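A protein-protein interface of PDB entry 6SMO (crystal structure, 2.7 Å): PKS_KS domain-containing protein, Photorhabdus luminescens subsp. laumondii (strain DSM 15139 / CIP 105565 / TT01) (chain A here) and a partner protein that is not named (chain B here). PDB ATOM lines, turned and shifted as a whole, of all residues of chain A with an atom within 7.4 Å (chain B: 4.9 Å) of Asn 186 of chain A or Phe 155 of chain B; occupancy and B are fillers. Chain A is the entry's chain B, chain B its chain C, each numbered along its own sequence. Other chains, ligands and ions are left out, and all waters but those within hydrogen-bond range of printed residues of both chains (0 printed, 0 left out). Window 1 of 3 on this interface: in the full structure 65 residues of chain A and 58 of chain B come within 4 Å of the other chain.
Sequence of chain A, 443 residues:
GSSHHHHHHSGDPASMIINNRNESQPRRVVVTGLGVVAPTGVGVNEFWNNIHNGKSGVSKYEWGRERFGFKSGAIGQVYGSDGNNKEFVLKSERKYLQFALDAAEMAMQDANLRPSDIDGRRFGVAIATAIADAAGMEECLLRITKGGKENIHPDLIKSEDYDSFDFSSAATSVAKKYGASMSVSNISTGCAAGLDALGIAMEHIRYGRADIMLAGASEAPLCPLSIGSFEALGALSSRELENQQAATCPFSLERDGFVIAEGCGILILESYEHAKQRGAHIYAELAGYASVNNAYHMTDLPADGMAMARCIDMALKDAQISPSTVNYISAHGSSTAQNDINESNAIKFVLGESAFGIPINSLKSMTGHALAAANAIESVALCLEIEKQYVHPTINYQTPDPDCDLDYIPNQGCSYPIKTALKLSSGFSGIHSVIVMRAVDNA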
ATOM      1  N   TYR A  96      40.489   0.972   8.604  1.00  0.00           N
ATOM      2  CA  TYR A  96      39.337   0.482   9.408  1.00  0.00           C
ATOM      3  C   TYR A  96      38.195   0.063   8.473  1.00  0.00           C
ATOM      4  O   TYR A  96      37.649  -1.043   8.653  1.00  0.00           O
ATOM      5  CB  TYR A  96      38.871   1.544  10.410  1.00  0.00           C
ATOM      6  CG  TYR A  96      37.487   1.309  10.961  1.00  0.00           C
ATOM      7  CD1 TYR A  96      37.197   0.172  11.699  1.00  0.00           C
ATOM      8  CD2 TYR A  96      36.459   2.212  10.734  1.00  0.00           C
ATOM      9  CE1 TYR A  96      35.926  -0.060  12.200  1.00  0.00           C
ATOM     10  CE2 TYR A  96      35.184   1.996  11.231  1.00  0.00           C
ATOM     11  CZ  TYR A  96      34.915   0.855  11.967  1.00  0.00           C
ATOM     12  OH  TYR A  96      33.661   0.633  12.459  1.00  0.00           O
ATOM     13  N   VAL A 125      23.626  -6.700   9.951  1.00  0.00           N
ATOM     14  CA  VAL A 125      25.100  -6.526  10.130  1.00  0.00           C
ATOM     15  C   VAL A 125      25.379  -6.142  11.589  1.00  0.00           C
ATOM     16  O   VAL A 125      24.518  -5.487  12.205  1.00  0.00           O
ATOM     17  CB  VAL A 125      25.661  -5.473   9.153  1.00  0.00           C
ATOM     18  CG1 VAL A 125      27.155  -5.253   9.339  1.00  0.00           C
ATOM     19  CG2 VAL A 125      25.358  -5.831   7.707  1.00  0.00           C
ATOM     20  N   ALA A 126      26.541  -6.548  12.110  1.00  0.00           N
ATOM     21  CA  ALA A 126      27.047  -6.197  13.459  1.00  0.00           C
ATOM     22  C   ALA A 126      28.581  -6.214  13.449  1.00  0.00           C
ATOM     23  O   ALA A 126      29.169  -7.224  13.880  1.00  0.00           O
ATOM     24  CB  ALA A 126      26.481  -7.147  14.486  1.00  0.00           C
ATOM     25  N   ILE A 127      29.197  -5.134  12.956  1.00  0.00           N
ATOM     26  CA  ILE A 127      30.678  -4.947  12.898  1.00  0.00           C
ATOM     27  C   ILE A 127      31.083  -3.971  14.006  1.00  0.00           C
ATOM     28  O   ILE A 127      30.686  -2.791  13.930  1.00  0.00           O
ATOM     29  CB  ILE A 127      31.130  -4.468  11.502  1.00  0.00           C
ATOM     30  CG1 ILE A 127      30.773  -5.491  10.419  1.00  0.00           C
ATOM     31  CG2 ILE A 127      32.617  -4.140  11.498  1.00  0.00           C
ATOM     32  CD1 ILE A 127      30.905  -4.973   9.006  1.00  0.00           C
ATOM     33  N   ALA A 128      31.849  -4.456  14.987  1.00  0.00           N
ATOM     34  CA  ALA A 128      32.281  -3.709  16.191  1.00  0.00           C
ATOM     35  C   ALA A 128      33.655  -3.073  15.955  1.00  0.00           C
ATOM     36  O   ALA A 128      34.351  -3.477  15.001  1.00  0.00           O
ATOM     37  CB  ALA A 128      32.308  -4.637  17.379  1.00  0.00           C
ATOM     38  N   THR A 129      34.021  -2.110  16.805  1.00  0.00           N
ATOM     39  CA  THR A 129      35.327  -1.398  16.785  1.00  0.00           C
ATOM     40  C   THR A 129      35.546  -0.714  18.138  1.00  0.00           C
ATOM     41  O   THR A 129      34.543  -0.342  18.776  1.00  0.00           O
ATOM     42  CB  THR A 129      35.387  -0.380  15.638  1.00  0.00           C
ATOM     43  OG1 THR A 129      36.752  -0.001  15.457  1.00  0.00           O
ATOM     44  CG2 THR A 129      34.540   0.849  15.885  1.00  0.00           C
ATOM     45  N   ALA A 130      36.804  -0.532  18.526  1.00  0.00           N
ATOM     46  CA  ALA A 130      37.148   0.165  19.780  1.00  0.00           C
ATOM     47  C   ALA A 130      37.396   1.654  19.496  1.00  0.00           C
ATOM     48  O   ALA A 130      36.884   2.469  20.269  1.00  0.00           O
ATOM     49  CB  ALA A 130      38.346  -0.499  20.404  1.00  0.00           C
ATOM     50  N   ALA A 132      37.446   2.880  15.911  1.00  0.00           N
ATOM     51  CA  ALA A 132      36.982   3.117  14.521  1.00  0.00           C
ATOM     52  C   ALA A 132      38.113   3.769  13.708  1.00  0.00           C
ATOM     53  O   ALA A 132      39.252   3.267  13.795  1.00  0.00           O
ATOM     54  CB  ALA A 132      35.723   3.951  14.541  1.00  0.00           C
ATOM     55  N   ASP A 166      32.566   9.125  11.763  1.00  0.00           N
ATOM     56  CA  ASP A 166      31.507   8.079  11.736  1.00  0.00           C
ATOM     57  C   ASP A 166      32.103   6.764  12.257  1.00  0.00           C
ATOM     58  O   ASP A 166      32.983   6.204  11.575  1.00  0.00           O
ATOM     59  CB  ASP A 166      30.914   7.925  10.331  1.00  0.00           C
ATOM     60  CG  ASP A 166      29.823   6.871  10.211  1.00  0.00           C
ATOM     61  OD1 ASP A 166      29.329   6.406  11.258  1.00  0.00           O
ATOM     62  OD2 ASP A 166      29.471   6.525   9.065  1.00  0.00           O
ATOM     63  N   PHE A 167      31.630   6.300  13.418  1.00  0.00           N
ATOM     64  CA  PHE A 167      32.087   5.060  14.103  1.00  0.00           C
ATOM     65  C   PHE A 167      31.575   3.824  13.354  1.00  0.00           C
ATOM     66  O   PHE A 167      32.319   2.825  13.284  1.00  0.00           O
ATOM     67  CB  PHE A 167      31.626   5.040  15.564  1.00  0.00           C
ATOM     68  CG  PHE A 167      32.738   5.040  16.584  1.00  0.00           C
ATOM     69  CD1 PHE A 167      33.421   6.207  16.895  1.00  0.00           C
ATOM     70  CD2 PHE A 167      33.096   3.872  17.241  1.00  0.00           C
ATOM     71  CE1 PHE A 167      34.439   6.201  17.837  1.00  0.00           C
ATOM     72  CE2 PHE A 167      34.113   3.869  18.182  1.00  0.00           C
ATOM     73  CZ  PHE A 167      34.783   5.033  18.478  1.00  0.00           C
ATOM     74  N   SER A 168      30.350   3.889  12.819  1.00  0.00           N
ATOM     75  CA  SER A 168      29.659   2.768  12.127  1.00  0.00           C
ATOM     76  C   SER A 168      29.791   2.908  10.604  1.00  0.00           C
ATOM     77  O   SER A 168      28.792   2.658   9.901  1.00  0.00           O
ATOM     78  CB  SER A 168      28.216   2.687  12.553  1.00  0.00           C
ATOM     79  OG  SER A 168      27.521   3.882  12.227  1.00  0.00           O
ATOM     80  N   SER A 169      30.978   3.283  10.115  1.00  0.00           N
ATOM     81  CA  SER A 169      31.322   3.338   8.669  1.00  0.00           C
ATOM     82  C   SER A 169      31.379   1.911   8.112  1.00  0.00           C
ATOM     83  O   SER A 169      30.828   1.680   7.019  1.00  0.00           O
ATOM     84  CB  SER A 169      32.622   4.063   8.435  1.00  0.00           C
ATOM     85  OG  SER A 169      32.514   5.429   8.803  1.00  0.00           O
ATOM     86  N   ALA A 170      32.017   1.002   8.856  1.00  0.00           N
ATOM     87  CA  ALA A 170      32.222  -0.422   8.500  1.00  0.00           C
ATOM     88  C   ALA A 170      30.871  -1.147   8.421  1.00  0.00           C
ATOM     89  O   ALA A 170      30.660  -1.883   7.438  1.00  0.00           O
ATOM     90  CB  ALA A 170      33.139  -1.071   9.507  1.00  0.00           C
ATOM     91  N   ALA A 171      29.998  -0.939   9.412  1.00  0.00           N
ATOM     92  CA  ALA A 171      28.688  -1.620   9.556  1.00  0.00           C
ATOM     93  C   ALA A 171      27.753  -1.235   8.402  1.00  0.00           C
ATOM     94  O   ALA A 171      27.150  -2.148   7.805  1.00  0.00           O
ATOM     95  CB  ALA A 171      28.074  -1.286  10.894  1.00  0.00           C
ATOM     96  N   THR A 172      27.641   0.063   8.104  1.00  0.00           N
ATOM     97  CA  THR A 172      26.685   0.632   7.113  1.00  0.00           C
ATOM     98  C   THR A 172      27.162   0.341   5.684  1.00  0.00           C
ATOM     99  O   THR A 172      26.299   0.041   4.834  1.00  0.00           O
ATOM    100  CB  THR A 172      26.477   2.134   7.337  1.00  0.00           C
ATOM    101  OG1 THR A 172      27.753   2.775   7.322  1.00  0.00           O
ATOM    102  CG2 THR A 172      25.767   2.440   8.637  1.00  0.00           C
ATOM    103  N   SER A 183      18.410  -5.088  11.544  1.00  0.00           N
ATOM    104  CA  SER A 183      19.247  -4.318  12.508  1.00  0.00           C
ATOM    105  C   SER A 183      20.711  -4.254  12.059  1.00  0.00           C
ATOM    106  O   SER A 183      21.342  -5.324  11.935  1.00  0.00           O
ATOM    107  CB  SER A 183      19.148  -4.912  13.890  1.00  0.00           C
ATOM    108  OG  SER A 183      20.101  -4.324  14.765  1.00  0.00           O
ATOM    109  N   VAL A 184      21.223  -3.036  11.841  1.00  0.00           N
ATOM    110  CA  VAL A 184      22.673  -2.730  11.652  1.00  0.00           C
ATOM    111  C   VAL A 184      23.152  -1.974  12.898  1.00  0.00           C
ATOM    112  O   VAL A 184      22.580  -0.906  13.190  1.00  0.00           O
ATOM    113  CB  VAL A 184      22.922  -1.923  10.362  1.00  0.00           C
ATOM    114  CG1 VAL A 184      24.378  -1.505  10.219  1.00  0.00           C
ATOM    115  CG2 VAL A 184      22.467  -2.687   9.128  1.00  0.00           C
ATOM    116  N   SER A 185      24.148  -2.514  13.607  1.00  0.00           N
ATOM    117  CA  SER A 185      24.645  -1.987  14.905  1.00  0.00           C
ATOM    118  C   SER A 185      26.173  -1.879  14.893  1.00  0.00           C
ATOM    119  O   SER A 185      26.819  -2.605  14.110  1.00  0.00           O
ATOM    120  CB  SER A 185      24.171  -2.843  16.053  1.00  0.00           C
ATOM    121  OG  SER A 185      24.668  -4.168  15.939  1.00  0.00           O
ATOM    122  N   ASN A 186      26.688  -1.010  15.763  1.00  0.00           N
ATOM    123  CA  ASN A 186      28.139  -0.815  15.996  1.00  0.00           C
ATOM    124  C   ASN A 186      28.369  -0.818  17.507  1.00  0.00           C
ATOM    125  O   ASN A 186      28.119   0.201  18.140  1.00  0.00           O
ATOM    126  CB  ASN A 186      28.696   0.457  15.354  1.00  0.00           C
ATOM    127  CG  ASN A 186      30.124   0.735  15.765  1.00  0.00           C
ATOM    128  OD1 ASN A 186      30.469   1.857  16.091  1.00  0.00           O
ATOM    129  ND2 ASN A 186      30.959  -0.283  15.765  1.00  0.00           N
ATOM    130  N   ILE A 187      28.753  -1.965  18.057  1.00  0.00           N
ATOM    131  CA  ILE A 187      29.062  -2.068  19.508  1.00  0.00           C
ATOM    132  C   ILE A 187      30.509  -1.604  19.668  1.00  0.00           C
ATOM    133  O   ILE A 187      31.349  -2.088  18.927  1.00  0.00           O
ATOM    134  CB  ILE A 187      28.817  -3.506  19.999  1.00  0.00           C
ATOM    135  CG1 ILE A 187      27.332  -3.858  19.913  1.00  0.00           C
ATOM    136  CG2 ILE A 187      29.354  -3.702  21.401  1.00  0.00           C
ATOM    137  CD1 ILE A 187      27.013  -5.283  20.243  1.00  0.00           C
ATOM    138  N   SER A 188      30.768  -0.680  20.587  1.00  0.00           N
ATOM    139  CA  SER A 188      32.134  -0.128  20.758  1.00  0.00           C
ATOM    140  C   SER A 188      32.664  -0.366  22.173  1.00  0.00           C
ATOM    141  O   SER A 188      33.362   0.505  22.677  1.00  0.00           O
ATOM    142  CB  SER A 188      32.180   1.317  20.383  1.00  0.00           C
ATOM    143  OG  SER A 188      31.210   2.048  21.102  1.00  0.00           O
ATOM    144  N   THR A 189      32.301  -1.487  22.788  1.00  0.00           N
ATOM    145  CA  THR A 189      32.731  -1.820  24.172  1.00  0.00           C
ATOM    146  C   THR A 189      34.220  -2.172  24.251  1.00  0.00           C
ATOM    147  O   THR A 189      34.525  -3.236  24.777  1.00  0.00           O
ATOM    148  CB  THR A 189      31.900  -2.983  24.716  1.00  0.00           C
ATOM    149  OG1 THR A 189      31.779  -3.924  23.653  1.00  0.00           O
ATOM    150  CG2 THR A 189      30.523  -2.556  25.164  1.00  0.00           C
ATOM    151  N   ALA A 193      34.177  -5.727  22.395  1.00  0.00           N
ATOM    152  CA  ALA A 193      33.234  -5.349  21.314  1.00  0.00           C
ATOM    153  C   ALA A 193      33.085  -6.487  20.296  1.00  0.00           C
ATOM    154  O   ALA A 193      31.945  -6.724  19.851  1.00  0.00           O
ATOM    155  CB  ALA A 193      33.713  -4.079  20.655  1.00  0.00           C
ATOM    156  N   ALA A 197      29.493  -8.138  19.580  1.00  0.00           N
ATOM    157  CA  ALA A 197      28.903  -8.095  18.221  1.00  0.00           C
ATOM    158  C   ALA A 197      28.402  -9.491  17.834  1.00  0.00           C
ATOM    159  O   ALA A 197      27.291  -9.588  17.278  1.00  0.00           O
ATOM    160  CB  ALA A 197      29.913  -7.574  17.230  1.00  0.00           C
ATOM    161  N   ILE A 200      25.220 -10.228  20.237  1.00  0.00           N
ATOM    162  CA  ILE A 200      23.948  -9.572  19.806  1.00  0.00           C
ATOM    163  C   ILE A 200      23.474 -10.216  18.494  1.00  0.00           C
ATOM    164  O   ILE A 200      22.248 -10.325  18.309  1.00  0.00           O
ATOM    165  CB  ILE A 200      24.105  -8.039  19.693  1.00  0.00           C
ATOM    166  CG1 ILE A 200      22.748  -7.330  19.752  1.00  0.00           C
ATOM    167  CG2 ILE A 200      24.891  -7.642  18.450  1.00  0.00           C
ATOM    168  CD1 ILE A 200      22.832  -5.871  20.133  1.00  0.00           C
ATOM    169  N   GLY A 216      31.248  -9.575  13.600  1.00  0.00           N
ATOM    170  CA  GLY A 216      32.711  -9.513  13.795  1.00  0.00           C
ATOM    171  C   GLY A 216      33.165  -8.150  14.288  1.00  0.00           C
ATOM    172  O   GLY A 216      32.371  -7.471  14.971  1.00  0.00           O
ATOM    173  N   SER A 218      36.441  -4.843  13.228  1.00  0.00           N
ATOM    174  CA  SER A 218      37.561  -4.283  12.434  1.00  0.00           C
ATOM    175  C   SER A 218      38.291  -3.242  13.281  1.00  0.00           C
ATOM    176  O   SER A 218      37.615  -2.499  13.949  1.00  0.00           O
ATOM    177  CB  SER A 218      37.061  -3.679  11.171  1.00  0.00           C
ATOM    178  OG  SER A 218      38.125  -3.254  10.358  1.00  0.00           O
ATOM    179  N   TYR B  99      23.448   0.482  29.721  1.00  0.00           N
ATOM    180  CA  TYR B  99      23.437   0.601  28.238  1.00  0.00           C
ATOM    181  C   TYR B  99      23.602   2.072  27.842  1.00  0.00           C
ATOM    182  O   TYR B  99      22.817   2.919  28.310  1.00  0.00           O
ATOM    183  CB  TYR B  99      22.169  -0.023  27.651  1.00  0.00           C
ATOM    184  CG  TYR B  99      22.333  -1.471  27.269  1.00  0.00           C
ATOM    185  CD1 TYR B  99      22.455  -2.454  28.238  1.00  0.00           C
ATOM    186  CD2 TYR B  99      22.393  -1.861  25.940  1.00  0.00           C
ATOM    187  CE1 TYR B  99      22.616  -3.788  27.899  1.00  0.00           C
ATOM    188  CE2 TYR B  99      22.554  -3.190  25.584  1.00  0.00           C
ATOM    189  CZ  TYR B  99      22.667  -4.158  26.567  1.00  0.00           C
ATOM    190  OH  TYR B  99      22.825  -5.469  26.226  1.00  0.00           O
ATOM    191  N   VAL B 100      24.625   2.360  27.033  1.00  0.00           N
ATOM    192  CA  VAL B 100      24.971   3.759  26.643  1.00  0.00           C
ATOM    193  C   VAL B 100      25.037   3.905  25.122  1.00  0.00           C
ATOM    194  O   VAL B 100      25.339   2.931  24.448  1.00  0.00           O
ATOM    195  CB  VAL B 100      26.314   4.174  27.279  1.00  0.00           C
ATOM    196  CG1 VAL B 100      26.606   5.658  27.176  1.00  0.00           C
ATOM    197  CG2 VAL B 100      26.433   3.719  28.719  1.00  0.00           C
ATOM    198  N   GLY B 101      24.691   5.097  24.636  1.00  0.00           N
ATOM    199  CA  GLY B 101      24.804   5.524  23.229  1.00  0.00           C
ATOM    200  C   GLY B 101      25.678   6.761  23.117  1.00  0.00           C
ATOM    201  O   GLY B 101      25.326   7.782  23.739  1.00  0.00           O
ATOM    202  N   ASN B 102      26.790   6.672  22.384  1.00  0.00           N
ATOM    203  CA  ASN B 102      27.757   7.787  22.201  1.00  0.00           C
ATOM    204  C   ASN B 102      28.512   7.594  20.883  1.00  0.00           C
ATOM    205  O   ASN B 102      29.063   6.495  20.679  1.00  0.00           O
ATOM    206  CB  ASN B 102      28.726   7.894  23.380  1.00  0.00           C
ATOM    207  CG  ASN B 102      29.711   9.033  23.221  1.00  0.00           C
ATOM    208  OD1 ASN B 102      30.908   8.804  23.071  1.00  0.00           O
ATOM    209  ND2 ASN B 102      29.214  10.259  23.231  1.00  0.00           N
ATOM    210  N   LYS B 153      26.633  -2.599  27.605  1.00  0.00           N
ATOM    211  CA  LYS B 153      27.168  -2.337  26.244  1.00  0.00           C
ATOM    212  C   LYS B 153      27.052  -0.864  25.856  1.00  0.00           C
ATOM    213  O   LYS B 153      26.238  -0.154  26.440  1.00  0.00           O
ATOM    214  CB  LYS B 153      26.392  -3.140  25.195  1.00  0.00           C
ATOM    215  CG  LYS B 153      26.273  -4.626  25.469  1.00  0.00           C
ATOM    216  CD  LYS B 153      27.611  -5.289  25.460  1.00  0.00           C
ATOM    217  CE  LYS B 153      27.788  -6.267  26.592  1.00  0.00           C
ATOM    218  NZ  LYS B 153      29.163  -6.176  27.124  1.00  0.00           N
ATOM    219  N   THR B 154      27.889  -0.449  24.908  1.00  0.00           N
ATOM    220  CA  THR B 154      27.896   0.926  24.355  1.00  0.00           C
ATOM    221  C   THR B 154      27.751   0.812  22.838  1.00  0.00           C
ATOM    222  O   THR B 154      28.418  -0.037  22.251  1.00  0.00           O
ATOM    223  CB  THR B 154      29.186   1.687  24.681  1.00  0.00           C
ATOM    224  OG1 THR B 154      29.399   1.703  26.087  1.00  0.00           O
ATOM    225  CG2 THR B 154      29.154   3.113  24.184  1.00  0.00           C
ATOM    226  N   PHE B 155      26.902   1.647  22.250  1.00  0.00           N
ATOM    227  CA  PHE B 155      26.681   1.663  20.788  1.00  0.00           C
ATOM    228  C   PHE B 155      27.178   3.005  20.268  1.00  0.00           C
ATOM    229  O   PHE B 155      26.977   3.997  20.951  1.00  0.00           O
ATOM    230  CB  PHE B 155      25.193   1.528  20.479  1.00  0.00           C
ATOM    231  CG  PHE B 155      24.600   0.190  20.823  1.00  0.00           C
ATOM    232  CD1 PHE B 155      24.189  -0.090  22.113  1.00  0.00           C
ATOM    233  CD2 PHE B 155      24.450  -0.785  19.856  1.00  0.00           C
ATOM    234  CE1 PHE B 155      23.640  -1.319  22.427  1.00  0.00           C
ATOM    235  CE2 PHE B 155      23.900  -2.014  20.171  1.00  0.00           C
ATOM    236  CZ  PHE B 155      23.495  -2.276  21.455  1.00  0.00           C
ATOM    237  N   SER B 156      27.822   3.004  19.104  1.00  0.00           N
ATOM    238  CA  SER B 156      28.323   4.256  18.487  1.00  0.00           C
ATOM    239  C   SER B 156      27.744   4.384  17.079  1.00  0.00           C
ATOM    240  O   SER B 156      28.287   5.153  16.296  1.00  0.00           O
ATOM    241  CB  SER B 156      29.818   4.281  18.467  1.00  0.00           C
ATOM    242  OG  SER B 156      30.337   4.239  19.783  1.00  0.00           O
ATOM    243  N   THR B 157      26.665   3.655  16.797  1.00  0.00           N
ATOM    244  CA  THR B 157      25.980   3.707  15.479  1.00  0.00           C
ATOM    245  C   THR B 157      25.474   5.135  15.252  1.00  0.00           C
ATOM    246  O   THR B 157      24.677   5.611  16.084  1.00  0.00           O
ATOM    247  CB  THR B 157      24.834   2.690  15.393  1.00  0.00           C
ATOM    248  OG1 THR B 157      25.254   1.472  16.008  1.00  0.00           O
ATOM    249  CG2 THR B 157      24.408   2.416  13.968  1.00  0.00           C
ATOM    250  N   ALA B 161      22.402   5.548  18.006  1.00  0.00           N
ATOM    251  CA  ALA B 161      23.200   4.831  19.032  1.00  0.00           C
ATOM    252  C   ALA B 161      22.366   4.650  20.307  1.00  0.00           C
ATOM    253  O   ALA B 161      22.233   3.500  20.771  1.00  0.00           O
ATOM    254  CB  ALA B 161      24.480   5.577  19.322  1.00  0.00           C
ATOM    255  N   GLN B 164      19.065   2.461  19.995  1.00  0.00           N
ATOM    256  CA  GLN B 164      19.381   1.010  20.084  1.00  0.00           C
ATOM    257  C   GLN B 164      19.668   0.637  21.545  1.00  0.00           C
ATOM    258  O   GLN B 164      19.248  -0.461  21.962  1.00  0.00           O
ATOM    259  CB  GLN B 164      20.564   0.659  19.177  1.00  0.00           C
ATOM    260  CG  GLN B 164      20.211   0.654  17.695  1.00  0.00           C
ATOM    261  CD  GLN B 164      21.383   0.321  16.803  1.00  0.00           C
ATOM    262  OE1 GLN B 164      22.544   0.481  17.176  1.00  0.00           O
ATOM    263  NE2 GLN B 164      21.085  -0.145  15.602  1.00  0.00           N
ATOM    264  N   ALA B 165      20.345   1.522  22.287  1.00  0.00           N
ATOM    265  CA  ALA B 165      20.765   1.319  23.695  1.00  0.00           C
ATOM    266  C   ALA B 165      19.548   0.991  24.572  1.00  0.00           C
ATOM    267  O   ALA B 165      19.648   0.044  25.375  1.00  0.00           O
ATOM    268  CB  ALA B 165      21.500   2.536  24.202  1.00  0.00           C
ATOM    269  N   TYR B 168      17.723  -2.625  23.287  1.00  0.00           N
ATOM    270  CA  TYR B 168      18.474  -3.874  23.587  1.00  0.00           C
ATOM    271  C   TYR B 168      18.659  -4.031  25.102  1.00  0.00           C
ATOM    272  O   TYR B 168      18.914  -5.167  25.548  1.00  0.00           O
ATOM    273  CB  TYR B 168      19.801  -3.903  22.823  1.00  0.00           C
ATOM    274  CG  TYR B 168      19.639  -4.109  21.338  1.00  0.00           C
ATOM    275  CD1 TYR B 168      19.110  -5.288  20.837  1.00  0.00           C
ATOM    276  CD2 TYR B 168      19.996  -3.124  20.432  1.00  0.00           C
ATOM    277  CE1 TYR B 168      18.945  -5.485  19.475  1.00  0.00           C
ATOM    278  CE2 TYR B 168      19.839  -3.305  19.067  1.00  0.00           C
ATOM    279  CZ  TYR B 168      19.312  -4.490  18.587  1.00  0.00           C
ATOM    280  OH  TYR B 168      19.156  -4.672  17.243  1.00  0.00           O
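Among the printed residues, merely in contact across the chains: Asn 186 of chain A with Phe 155 of chain B (3.3 Å), Thr 189 of chain A with Thr 154 of chain B (3.4 Å), Phe 167 of chain A with Ser 156 of chain B (3.4 Å), Ile 187 of chain A with Thr 154 of chain B (3.5 Å), Thr 189 of chain A with Lys 153 of chain B (3.5 Å), Ser 168 of chain A with Thr 157 of chain B (3.6 Å), Ser 185 of chain A with Thr 157 of chain B (3.6 Å), Ile 200 of chain A with Tyr 168 of chain B (3.8 Å), Ser 185 of chain A with Gln 164 of chain B (3.9 Å), Val 184 of chain A with Thr 157 of chain B (3.9 Å), Ile 200 of chain A with Phe 155 of chain B (3.9 Å) and Ile 187 of chain A with Phe 155 of chain B (3.9 Å).
The backbone NH (N) of Asn 186 of chain A lies within hydrogen-bond range of the side-chain hydroxyl (OG1) of Thr 157 of chain B, 2.9 Å away.
OG of Ser 188 of chain A lies within hydrogen-bond range of OG of Ser 156 of chain B, 2.7 Å away.
O of Val 184 of chain A is in hydrogen-bond range of NE2 of Gln 164 of chain B, 2.9 Å away.
The side-chain hydroxyl of Ser 183 of chain A lies within hydrogen-bond range of the side-chain hydroxyl of Tyr 168 of chain B (2.7 Å).
The backbone NH of Ser 188 of chain A sits at hydrogen-bond distance from the backbone carbonyl oxygen of Thr 154 of chain B (3.0 Å).
The backbone carbonyl oxygen (O) of Asn 186 of chain A sits at hydrogen-bond distance from the backbone NH (N) of Ser 156 of chain B.
Asn 186 of chain A touches three residues of chain B.
Of chain A, only Asn 186 (3.3 Å), Ile 187 (3.9 Å) and Ile 200 (3.9 Å) come within 4 Å of Phe 155 of chain B.
Printed residues of chain A within 4 Å of Lys 153 of chain B: Thr 189 (3.5 Å).
Of the printed residues of chain A, Thr 157 of chain B touches Ser 168, Val 184, Ser 185 and Asn 186.
Of the printed residues of chain B, Ile 200 of chain A touches Phe 155 (3.9 Å) and Tyr 168 (3.8 Å).
Of the printed residues of chain B, Ser 185 of chain A touches Thr 157 (3.6 Å) and Gln 164 (3.9 Å).
Ala 193 of chain A touches none of the printed residues of chain B.
Gly 101 of chain B touches none of the printed residues of chain A.
The nearest residue of chain B that does not touch Asn 186 of chain A is Thr 154 of chain B (4.1 Å).
The nearest printed residue of chain A that does not touch Phe 155 of chain B is Ser 185 of chain A (4.2 Å).
The backbone NH (N) of Val 100 of chain B sits at hydrogen-bond distance from the backbone carbonyl oxygen (O) of Lys 153 of chain B (3.0 Å).
The backbone NH (N) of Asn 102 of chain B sits at hydrogen-bond distance from the backbone carbonyl oxygen (O) of Phe 155 of chain B, 3.0 Å away.
The backbone NH of Thr 129 of chain A lies within hydrogen-bond range of the backbone carbonyl oxygen of Ile 187 of chain A, 3.4 Å away.
The backbone carbonyl oxygen (O) of Asn 102 of chain B lies within hydrogen-bond range of the side-chain hydroxyl (OG) of Ser 156 of chain B.
The side-chain hydroxyl (OG1) of Thr 189 of chain A sits close to the backbone NH (N) of Ala 193 of chain A (3.3 Å).
O of Phe 167 of chain A lies close to OD1 of Asn 186 of chain A, 3.5 Å away.
Of the 27 printed residues of chain A, 10 touch a printed residue of chain B.
Printed residues of chain A that touch a printed residue of chain B: Phe 167, Ser 168, Ser 183, Val 184, Ser 185, Asn 186, Ile 187, Ser 188, Thr 189 and Ile 200.
Hydrophobic or aromatic side chains of chain A within 4 Å of the printed part of chain B: Phe 167, Ile 187 and Ile 200.
Of the 13 printed residues of chain B, 7 touch a printed residue of chain A.
Hydrophobic or aromatic side chains of chain B within 4 Å of the printed part of chain A: Phe 155 and Tyr 168.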
